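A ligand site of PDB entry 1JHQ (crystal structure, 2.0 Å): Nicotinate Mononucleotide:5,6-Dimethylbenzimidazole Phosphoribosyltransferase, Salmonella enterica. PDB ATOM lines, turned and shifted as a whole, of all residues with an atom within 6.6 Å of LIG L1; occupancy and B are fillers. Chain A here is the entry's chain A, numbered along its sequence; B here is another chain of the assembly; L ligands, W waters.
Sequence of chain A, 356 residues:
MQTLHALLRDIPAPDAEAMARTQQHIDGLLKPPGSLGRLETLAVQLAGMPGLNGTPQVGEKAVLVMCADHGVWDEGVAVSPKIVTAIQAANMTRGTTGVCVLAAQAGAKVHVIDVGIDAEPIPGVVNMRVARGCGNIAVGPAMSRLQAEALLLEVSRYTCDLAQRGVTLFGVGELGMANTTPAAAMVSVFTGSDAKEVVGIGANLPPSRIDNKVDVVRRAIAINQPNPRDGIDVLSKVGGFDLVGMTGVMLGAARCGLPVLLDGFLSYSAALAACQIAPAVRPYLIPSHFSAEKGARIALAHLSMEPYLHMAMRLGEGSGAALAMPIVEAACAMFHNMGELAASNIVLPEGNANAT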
ATOM      1  N   GLU A 174      31.892 -25.970 -26.427  1.00  0.00           N
ATOM      2  CA  GLU A 174      31.743 -27.411 -26.527  1.00  0.00           C
ATOM      3  C   GLU A 174      30.289 -27.853 -26.449  1.00  0.00           C
ATOM      4  O   GLU A 174      29.374 -27.040 -26.251  1.00  0.00           O
ATOM      5  CB  GLU A 174      32.569 -28.138 -25.442  1.00  0.00           C
ATOM      6  CG  GLU A 174      32.402 -27.545 -24.002  1.00  0.00           C
ATOM      7  CD  GLU A 174      30.939 -27.431 -23.571  1.00  0.00           C
ATOM      8  OE1 GLU A 174      30.215 -28.385 -23.403  1.00  0.00           O
ATOM      9  OE2 GLU A 174      30.520 -26.177 -23.501  1.00  0.00           O
ATOM     10  N   ASN A 179      30.219 -34.269 -20.204  1.00  0.00           N
ATOM     11  CA  ASN A 179      31.529 -33.605 -20.228  1.00  0.00           C
ATOM     12  C   ASN A 179      32.028 -32.916 -18.957  1.00  0.00           C
ATOM     13  O   ASN A 179      33.237 -32.689 -18.794  1.00  0.00           O
ATOM     14  CB  ASN A 179      31.830 -32.862 -21.559  1.00  0.00           C
ATOM     15  CG  ASN A 179      31.096 -31.541 -21.742  1.00  0.00           C
ATOM     16  OD1 ASN A 179      30.368 -31.083 -20.833  1.00  0.00           O
ATOM     17  ND2 ASN A 179      31.296 -30.921 -22.909  1.00  0.00           N
ATOM     18  N   THR A 180      31.117 -32.568 -18.031  1.00  0.00           N
ATOM     19  CA  THR A 180      31.521 -31.921 -16.789  1.00  0.00           C
ATOM     20  C   THR A 180      32.265 -32.886 -15.863  1.00  0.00           C
ATOM     21  O   THR A 180      33.002 -32.491 -14.935  1.00  0.00           O
ATOM     22  CB  THR A 180      30.383 -31.118 -16.099  1.00  0.00           C
ATOM     23  OG1 THR A 180      29.372 -31.992 -15.621  1.00  0.00           O
ATOM     24  CG2 THR A 180      29.755 -30.131 -17.070  1.00  0.00           C
ATOM     25  N   ILE A 201      26.985 -29.836 -10.447  1.00  0.00           N
ATOM     26  CA  ILE A 201      25.761 -30.461 -10.915  1.00  0.00           C
ATOM     27  C   ILE A 201      25.663 -30.538 -12.447  1.00  0.00           C
ATOM     28  O   ILE A 201      24.725 -31.132 -13.002  1.00  0.00           O
ATOM     29  CB  ILE A 201      24.502 -29.854 -10.256  1.00  0.00           C
ATOM     30  N   GLY A 202      26.624 -29.917 -13.139  1.00  0.00           N
ATOM     31  CA  GLY A 202      26.572 -29.947 -14.595  1.00  0.00           C
ATOM     32  C   GLY A 202      25.205 -29.463 -15.136  1.00  0.00           C
ATOM     33  O   GLY A 202      24.638 -28.424 -14.743  1.00  0.00           O
ATOM     34  N   ALA A 203      24.658 -30.229 -16.052  1.00  0.00           N
ATOM     35  CA  ALA A 203      23.380 -29.874 -16.650  1.00  0.00           C
ATOM     36  C   ALA A 203      22.245 -30.421 -15.797  1.00  0.00           C
ATOM     37  O   ALA A 203      21.566 -31.380 -16.154  1.00  0.00           O
ATOM     38  CB  ALA A 203      23.258 -30.314 -18.112  1.00  0.00           C
ATOM     39  N   ASN A 204      22.055 -29.797 -14.642  1.00  0.00           N
ATOM     40  CA  ASN A 204      20.980 -30.179 -13.740  1.00  0.00           C
ATOM     41  C   ASN A 204      21.056 -31.592 -13.154  1.00  0.00           C
ATOM     42  O   ASN A 204      20.043 -32.265 -13.050  1.00  0.00           O
ATOM     43  CB  ASN A 204      19.582 -29.883 -14.322  1.00  0.00           C
ATOM     44  CG  ASN A 204      19.360 -28.409 -14.597  1.00  0.00           C
ATOM     45  OD1 ASN A 204      19.865 -27.545 -13.836  1.00  0.00           O
ATOM     46  ND2 ASN A 204      18.633 -28.101 -15.682  1.00  0.00           N
ATOM     47  N   ASP A 263      35.166 -19.644 -22.164  1.00  0.00           N
ATOM     48  CA  ASP A 263      33.745 -19.739 -21.928  1.00  0.00           C
ATOM     49  C   ASP A 263      33.545 -20.002 -20.420  1.00  0.00           C
ATOM     50  O   ASP A 263      33.919 -19.177 -19.604  1.00  0.00           O
ATOM     51  CB  ASP A 263      33.035 -20.775 -22.852  1.00  0.00           C
ATOM     52  CG  ASP A 263      31.514 -20.740 -22.747  1.00  0.00           C
ATOM     53  OD1 ASP A 263      30.868 -19.737 -22.472  1.00  0.00           O
ATOM     54  OD2 ASP A 263      30.949 -21.899 -22.920  1.00  0.00           O
ATOM     55  N   GLY A 264      33.001 -21.170 -20.089  1.00  0.00           N
ATOM     56  CA  GLY A 264      32.782 -21.559 -18.717  1.00  0.00           C
ATOM     57  C   GLY A 264      33.694 -22.687 -18.219  1.00  0.00           C
ATOM     58  O   GLY A 264      34.853 -22.847 -18.627  1.00  0.00           O
ATOM     59  N   PHE A 265      33.130 -23.462 -17.298  1.00  0.00           N
ATOM     60  CA  PHE A 265      33.832 -24.564 -16.654  1.00  0.00           C
ATOM     61  C   PHE A 265      34.611 -25.506 -17.566  1.00  0.00           C
ATOM     62  O   PHE A 265      35.777 -25.818 -17.290  1.00  0.00           O
ATOM     63  CB  PHE A 265      32.854 -25.362 -15.760  1.00  0.00           C
ATOM     64  CG  PHE A 265      33.596 -26.270 -14.839  1.00  0.00           C
ATOM     65  CD1 PHE A 265      33.436 -27.657 -14.901  1.00  0.00           C
ATOM     66  CD2 PHE A 265      34.499 -25.739 -13.907  1.00  0.00           C
ATOM     67  CE1 PHE A 265      34.161 -28.493 -14.042  1.00  0.00           C
ATOM     68  CE2 PHE A 265      35.219 -26.563 -13.044  1.00  0.00           C
ATOM     69  CZ  PHE A 265      35.044 -27.953 -13.113  1.00  0.00           C
ATOM     70  N   LEU A 266      33.963 -26.019 -18.623  1.00  0.00           N
ATOM     71  CA  LEU A 266      34.639 -26.940 -19.524  1.00  0.00           C
ATOM     72  C   LEU A 266      35.883 -26.244 -20.077  1.00  0.00           C
ATOM     73  O   LEU A 266      36.975 -26.808 -20.180  1.00  0.00           O
ATOM     74  CB  LEU A 266      33.779 -27.392 -20.734  1.00  0.00           C
ATOM     75  CG  LEU A 266      32.617 -28.331 -20.416  1.00  0.00           C
ATOM     76  CD1 LEU A 266      32.998 -29.317 -19.316  1.00  0.00           C
ATOM     77  CD2 LEU A 266      31.371 -27.535 -20.019  1.00  0.00           C
ATOM     78  N   SER A 267      35.704 -24.977 -20.418  1.00  0.00           N
ATOM     79  CA  SER A 267      36.800 -24.216 -20.980  1.00  0.00           C
ATOM     80  C   SER A 267      37.909 -23.972 -19.986  1.00  0.00           C
ATOM     81  O   SER A 267      39.078 -23.975 -20.376  1.00  0.00           O
ATOM     82  CB  SER A 267      36.360 -22.954 -21.692  1.00  0.00           C
ATOM     83  OG  SER A 267      36.170 -21.922 -20.749  1.00  0.00           O
ATOM     84  N   TYR A 268      37.567 -23.775 -18.703  1.00  0.00           N
ATOM     85  CA  TYR A 268      38.656 -23.585 -17.740  1.00  0.00           C
ATOM     86  C   TYR A 268      39.516 -24.830 -17.698  1.00  0.00           C
ATOM     87  O   TYR A 268      40.728 -24.744 -17.627  1.00  0.00           O
ATOM     88  CB  TYR A 268      38.203 -23.297 -16.298  1.00  0.00           C
ATOM     89  CG  TYR A 268      37.142 -22.245 -16.158  1.00  0.00           C
ATOM     90  CD1 TYR A 268      36.261 -22.321 -15.075  1.00  0.00           C
ATOM     91  CD2 TYR A 268      36.997 -21.183 -17.064  1.00  0.00           C
ATOM     92  CE1 TYR A 268      35.233 -21.401 -14.893  1.00  0.00           C
ATOM     93  CE2 TYR A 268      35.987 -20.236 -16.891  1.00  0.00           C
ATOM     94  CZ  TYR A 268      35.110 -20.357 -15.810  1.00  0.00           C
ATOM     95  OH  TYR A 268      34.082 -19.470 -15.627  1.00  0.00           O
ATOM     96  N   HIS A 289      33.029 -15.146 -18.597  1.00  0.00           N
ATOM     97  CA  HIS A 289      32.177 -15.103 -17.436  1.00  0.00           C
ATOM     98  C   HIS A 289      32.570 -16.069 -16.355  1.00  0.00           C
ATOM     99  O   HIS A 289      33.443 -16.908 -16.549  1.00  0.00           O
ATOM    100  CB  HIS A 289      30.714 -15.312 -17.849  1.00  0.00           C
ATOM    101  CG  HIS A 289      30.415 -16.755 -18.081  1.00  0.00           C
ATOM    102  ND1 HIS A 289      31.022 -17.471 -19.112  1.00  0.00           N
ATOM    103  CD2 HIS A 289      29.606 -17.597 -17.391  1.00  0.00           C
ATOM    104  CE1 HIS A 289      30.541 -18.726 -19.045  1.00  0.00           C
ATOM    105  NE2 HIS A 289      29.698 -18.833 -18.012  1.00  0.00           N
ATOM    106  N   SER A 291      31.458 -19.040 -14.426  1.00  0.00           N
ATOM    107  CA  SER A 291      30.539 -20.177 -14.448  1.00  0.00           C
ATOM    108  C   SER A 291      29.935 -20.507 -13.078  1.00  0.00           C
ATOM    109  O   SER A 291      30.635 -20.481 -12.079  1.00  0.00           O
ATOM    110  CB  SER A 291      31.212 -21.436 -15.001  1.00  0.00           C
ATOM    111  OG  SER A 291      30.406 -22.586 -14.757  1.00  0.00           O
ATOM    112  N   ALA A 292      28.659 -20.875 -13.058  1.00  0.00           N
ATOM    113  CA  ALA A 292      28.000 -21.281 -11.822  1.00  0.00           C
ATOM    114  C   ALA A 292      28.361 -22.719 -11.392  1.00  0.00           C
ATOM    115  O   ALA A 292      27.863 -23.194 -10.387  1.00  0.00           O
ATOM    116  CB  ALA A 292      26.485 -21.096 -11.924  1.00  0.00           C
ATOM    117  N   GLU A 293      29.235 -23.420 -12.137  1.00  0.00           N
ATOM    118  CA  GLU A 293      29.672 -24.755 -11.731  1.00  0.00           C
ATOM    119  C   GLU A 293      30.484 -24.618 -10.412  1.00  0.00           C
ATOM    120  O   GLU A 293      31.286 -23.708 -10.228  1.00  0.00           O
ATOM    121  CB  GLU A 293      30.453 -25.496 -12.878  1.00  0.00           C
ATOM    122  CG  GLU A 293      30.897 -26.931 -12.565  1.00  0.00           C
ATOM    123  CD  GLU A 293      29.879 -28.011 -12.888  1.00  0.00           C
ATOM    124  OE1 GLU A 293      28.679 -27.792 -13.030  1.00  0.00           O
ATOM    125  OE2 GLU A 293      30.429 -29.204 -12.943  1.00  0.00           O
ATOM    126  N   MET A 313      25.821 -18.189 -15.255  1.00  0.00           N
ATOM    127  CA  MET A 313      25.597 -19.040 -16.406  1.00  0.00           C
ATOM    128  C   MET A 313      26.265 -20.410 -16.293  1.00  0.00           C
ATOM    129  O   MET A 313      27.349 -20.570 -15.689  1.00  0.00           O
ATOM    130  CB  MET A 313      25.931 -18.333 -17.733  1.00  0.00           C
ATOM    131  CG  MET A 313      24.837 -17.363 -18.194  1.00  0.00           C
ATOM    132  SD  MET A 313      25.480 -16.143 -19.369  1.00  0.00           S
ATOM    133  CE  MET A 313      26.235 -17.211 -20.618  1.00  0.00           C
ATOM    134  N   ARG A 314      25.578 -21.421 -16.865  1.00  0.00           N
ATOM    135  CA  ARG A 314      26.060 -22.805 -16.847  1.00  0.00           C
ATOM    136  C   ARG A 314      25.499 -23.591 -18.031  1.00  0.00           C
ATOM    137  O   ARG A 314      25.035 -24.721 -17.892  1.00  0.00           O
ATOM    138  CB  ARG A 314      25.667 -23.472 -15.536  1.00  0.00           C
ATOM    139  CG  ARG A 314      24.189 -23.256 -15.223  1.00  0.00           C
ATOM    140  CD  ARG A 314      23.861 -23.880 -13.874  1.00  0.00           C
ATOM    141  NE  ARG A 314      22.472 -23.741 -13.456  1.00  0.00           N
ATOM    142  CZ  ARG A 314      21.451 -24.502 -13.842  1.00  0.00           C
ATOM    143  NH1 ARG A 314      21.600 -25.493 -14.721  1.00  0.00           N
ATOM    144  NH2 ARG A 314      20.242 -24.268 -13.338  1.00  0.00           N
ATOM    145  N   LEU A 315      25.533 -22.986 -19.202  1.00  0.00           N
ATOM    146  CA  LEU A 315      25.051 -23.631 -20.380  1.00  0.00           C
ATOM    147  C   LEU A 315      26.182 -24.267 -21.205  1.00  0.00           C
ATOM    148  O   LEU A 315      25.998 -25.344 -21.786  1.00  0.00           O
ATOM    149  CB  LEU A 315      24.264 -22.630 -21.274  1.00  0.00           C
ATOM    150  CG  LEU A 315      23.832 -23.142 -22.675  1.00  0.00           C
ATOM    151  CD1 LEU A 315      22.891 -24.338 -22.536  1.00  0.00           C
ATOM    152  CD2 LEU A 315      23.102 -22.020 -23.446  1.00  0.00           C
ATOM    153  N   GLY A 316      27.313 -23.566 -21.323  1.00  0.00           N
ATOM    154  CA  GLY A 316      28.373 -24.055 -22.187  1.00  0.00           C
ATOM    155  C   GLY A 316      28.064 -23.601 -23.618  1.00  0.00           C
ATOM    156  O   GLY A 316      27.372 -22.567 -23.846  1.00  0.00           O
ATOM    157  N   GLU A 317      28.569 -24.369 -24.594  1.00  0.00           N
ATOM    158  CA  GLU A 317      28.396 -24.106 -26.037  1.00  0.00           C
ATOM    159  C   GLU A 317      29.220 -22.936 -26.536  1.00  0.00           C
ATOM    160  O   GLU A 317      29.260 -22.672 -27.735  1.00  0.00           O
ATOM    161  CB  GLU A 317      26.924 -23.780 -26.389  1.00  0.00           C
ATOM    162  CG  GLU A 317      25.900 -24.794 -25.829  1.00  0.00           C
ATOM    163  CD  GLU A 317      24.529 -24.556 -26.402  1.00  0.00           C
ATOM    164  OE1 GLU A 317      24.271 -23.597 -27.103  1.00  0.00           O
ATOM    165  OE2 GLU A 317      23.657 -25.487 -26.104  1.00  0.00           O
ATOM    166  N   GLY A 318      29.841 -22.213 -25.619  1.00  0.00           N
ATOM    167  CA  GLY A 318      30.572 -21.035 -25.974  1.00  0.00           C
ATOM    168  C   GLY A 318      29.651 -19.816 -25.816  1.00  0.00           C
ATOM    169  O   GLY A 318      29.913 -18.719 -26.317  1.00  0.00           O
ATOM    170  N   SER A 319      28.531 -19.997 -25.093  1.00  0.00           N
ATOM    171  CA  SER A 319      27.572 -18.910 -24.896  1.00  0.00           C
ATOM    172  C   SER A 319      28.136 -17.685 -24.140  1.00  0.00           C
ATOM    173  O   SER A 319      27.857 -16.543 -24.531  1.00  0.00           O
ATOM    174  CB  SER A 319      26.268 -19.400 -24.294  1.00  0.00           C
ATOM    175  OG  SER A 319      26.587 -20.157 -23.138  1.00  0.00           O
ATOM    176  N   PRO B  32      19.184 -26.718 -20.908  1.00  0.00           N
ATOM    177  CA  PRO B  32      18.749 -27.222 -19.606  1.00  0.00           C
ATOM    178  C   PRO B  32      18.076 -26.071 -18.847  1.00  0.00           C
ATOM    179  O   PRO B  32      18.578 -24.940 -18.815  1.00  0.00           O
ATOM    180  CB  PRO B  32      20.021 -27.674 -18.862  1.00  0.00           C
ATOM    181  CG  PRO B  32      21.150 -27.648 -19.895  1.00  0.00           C
ATOM    182  CD  PRO B  32      20.630 -26.984 -21.162  1.00  0.00           C
HETATM  183  N1  LIG L   1      27.599 -27.106 -19.118  1.00  0.00           N
HETATM  184  C1  LIG L   1      28.475 -26.073 -19.230  1.00  0.00           C
HETATM  185  C2  LIG L   1      28.848 -25.386 -18.087  1.00  0.00           C
HETATM  186  C3  LIG L   1      28.348 -25.761 -16.788  1.00  0.00           C
HETATM  187  C4  LIG L   1      27.459 -26.844 -16.814  1.00  0.00           C
HETATM  188  C5  LIG L   1      27.049 -27.555 -17.911  1.00  0.00           C
HETATM  189  C6  LIG L   1      29.815 -24.226 -18.210  1.00  0.00           C
HETATM  190  O1  LIG L   1      30.158 -23.588 -17.158  1.00  0.00           O
HETATM  191  O2  LIG L   1      30.284 -23.906 -19.346  1.00  0.00           O
HETATM  192  N1  LG2 L   2      24.145 -27.281 -24.351  1.00  0.00           N
HETATM  193  N2  LG2 L   2      25.038 -28.323 -22.556  1.00  0.00           N
HETATM  194  C1  LG2 L   2      25.183 -27.369 -23.513  1.00  0.00           C
HETATM  195  C2  LG2 L   2      23.764 -28.886 -22.855  1.00  0.00           C
HETATM  196  C3  LG2 L   2      23.223 -28.219 -23.935  1.00  0.00           C
HETATM  197  C4  LG2 L   2      21.939 -28.532 -24.400  1.00  0.00           C
HETATM  198  C5  LG2 L   2      21.219 -29.561 -23.826  1.00  0.00           C
HETATM  199  C6  LG2 L   2      21.770 -30.238 -22.709  1.00  0.00           C
HETATM  200  C7  LG2 L   2      23.034 -29.916 -22.247  1.00  0.00           C
HETATM  201  O1  LG2 L   2      19.948 -30.005 -24.117  1.00  0.00           O
HETATM  202  C8  LG2 L   2      19.364 -29.247 -25.161  1.00  0.00           C
HETATM  203  P1  LG2 L   2      26.670 -32.780 -18.001  1.00  0.00           P
HETATM  204  O2  LG2 L   2      28.080 -33.020 -17.598  1.00  0.00           O
HETATM  205  O3  LG2 L   2      25.769 -32.817 -16.827  1.00  0.00           O
HETATM  206  O4  LG2 L   2      26.108 -33.584 -19.136  1.00  0.00           O
HETATM  207  O5  LG2 L   2      26.758 -31.232 -18.496  1.00  0.00           O
HETATM  208  C9  LG2 L   2      27.560 -30.871 -19.632  1.00  0.00           C
HETATM  209  C10 LG2 L   2      26.672 -30.865 -20.873  1.00  0.00           C
HETATM  210  O6  LG2 L   2      25.643 -29.828 -20.724  1.00  0.00           O
HETATM  211  C11 LG2 L   2      27.407 -30.505 -22.162  1.00  0.00           C
HETATM  212  O7  LG2 L   2      26.671 -30.861 -23.347  1.00  0.00           O
HETATM  213  C12 LG2 L   2      27.411 -28.978 -21.991  1.00  0.00           C
HETATM  214  O8  LG2 L   2      27.676 -28.389 -23.290  1.00  0.00           O
HETATM  215  C13 LG2 L   2      25.998 -28.667 -21.477  1.00  0.00           C
HETATM  216  O   HOH W   1      32.725 -24.038 -20.740  1.00  0.00           O
HETATM  217  O   HOH W   2      29.585 -21.489 -20.376  1.00  0.00           O
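Merely in contact with LIG L1: Leu 266 (3.3 Å), Arg 314 (3.4 Å), Gly 316 (3.4 Å), Gly 264 (3.5 Å), Leu 315 (3.5 Å), Thr 180 (3.8 Å) and Gly 202 (3.8 Å). Within 4 Å of LIG L1: Thr 180, Gly 202, Gly 264, Phe 265, Leu 266, Ser 291, Arg 314, Leu 315 and Gly 316. The nearest printed residue that does not touch LIG L1 is Ala 203 (4.04 Å).
N of Gly 202 lies within hydrogen-bond range of OE1 of Glu 293 (3.0 Å). The backbone carbonyl oxygen (O) of Gly 316 lies within hydrogen-bond range of the side-chain hydroxyl (OG) of Ser 319 (2.6 Å). The guanidinium group of Arg 314 is in hydrogen-bond range of the side-chain amide oxygen of Asn 204, 2.8 Å away. OG of Ser 291 lies within hydrogen-bond range of N of Glu 293, 3.0 Å away. N of Ser 291 is in hydrogen-bond range of OH of Tyr 268, at 2.9 Å. The backbone carbonyl oxygen (O) of Gly 264 lies within hydrogen-bond range of the side-chain hydroxyl (OG) of Ser 267.
An oxygen (O2) of LG2 L2 sits at hydrogen-bond distance from the backbone NH (N) of Thr 180, at 3.1 Å. An oxygen (O1) of LIG L1 lies within hydrogen-bond range of the backbone NH of Phe 265 (3.0 Å). The side-chain carboxylate (OE1) of Glu 174 is in hydrogen-bond range of an oxygen (O8) of LG2 L2, at 2.5 Å. A nitrogen (N1) of LG2 L2 lies within hydrogen-bond range of the side-chain carboxylate (OE2) of Glu 317, at 2.6 Å. OG1 of Thr 180 is in hydrogen-bond range of O2 of LG2 L2, 2.6 Å away. An oxygen (O1) of LIG L1 is in hydrogen-bond range of the side-chain hydroxyl of Ser 291 (2.6 Å). An oxygen (O3) of LG2 L2 lies within hydrogen-bond range of the backbone NH of Ala 203, 2.9 Å away.
Water W2 lies within hydrogen-bond range of an oxygen (O2) of LIG L1 (2.7 Å), the side-chain carboxylate of Asp 263 (2.9 Å), the backbone NH of Gly 316 (3.2 Å) and the backbone NH of Gly 264 (3.4 Å).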
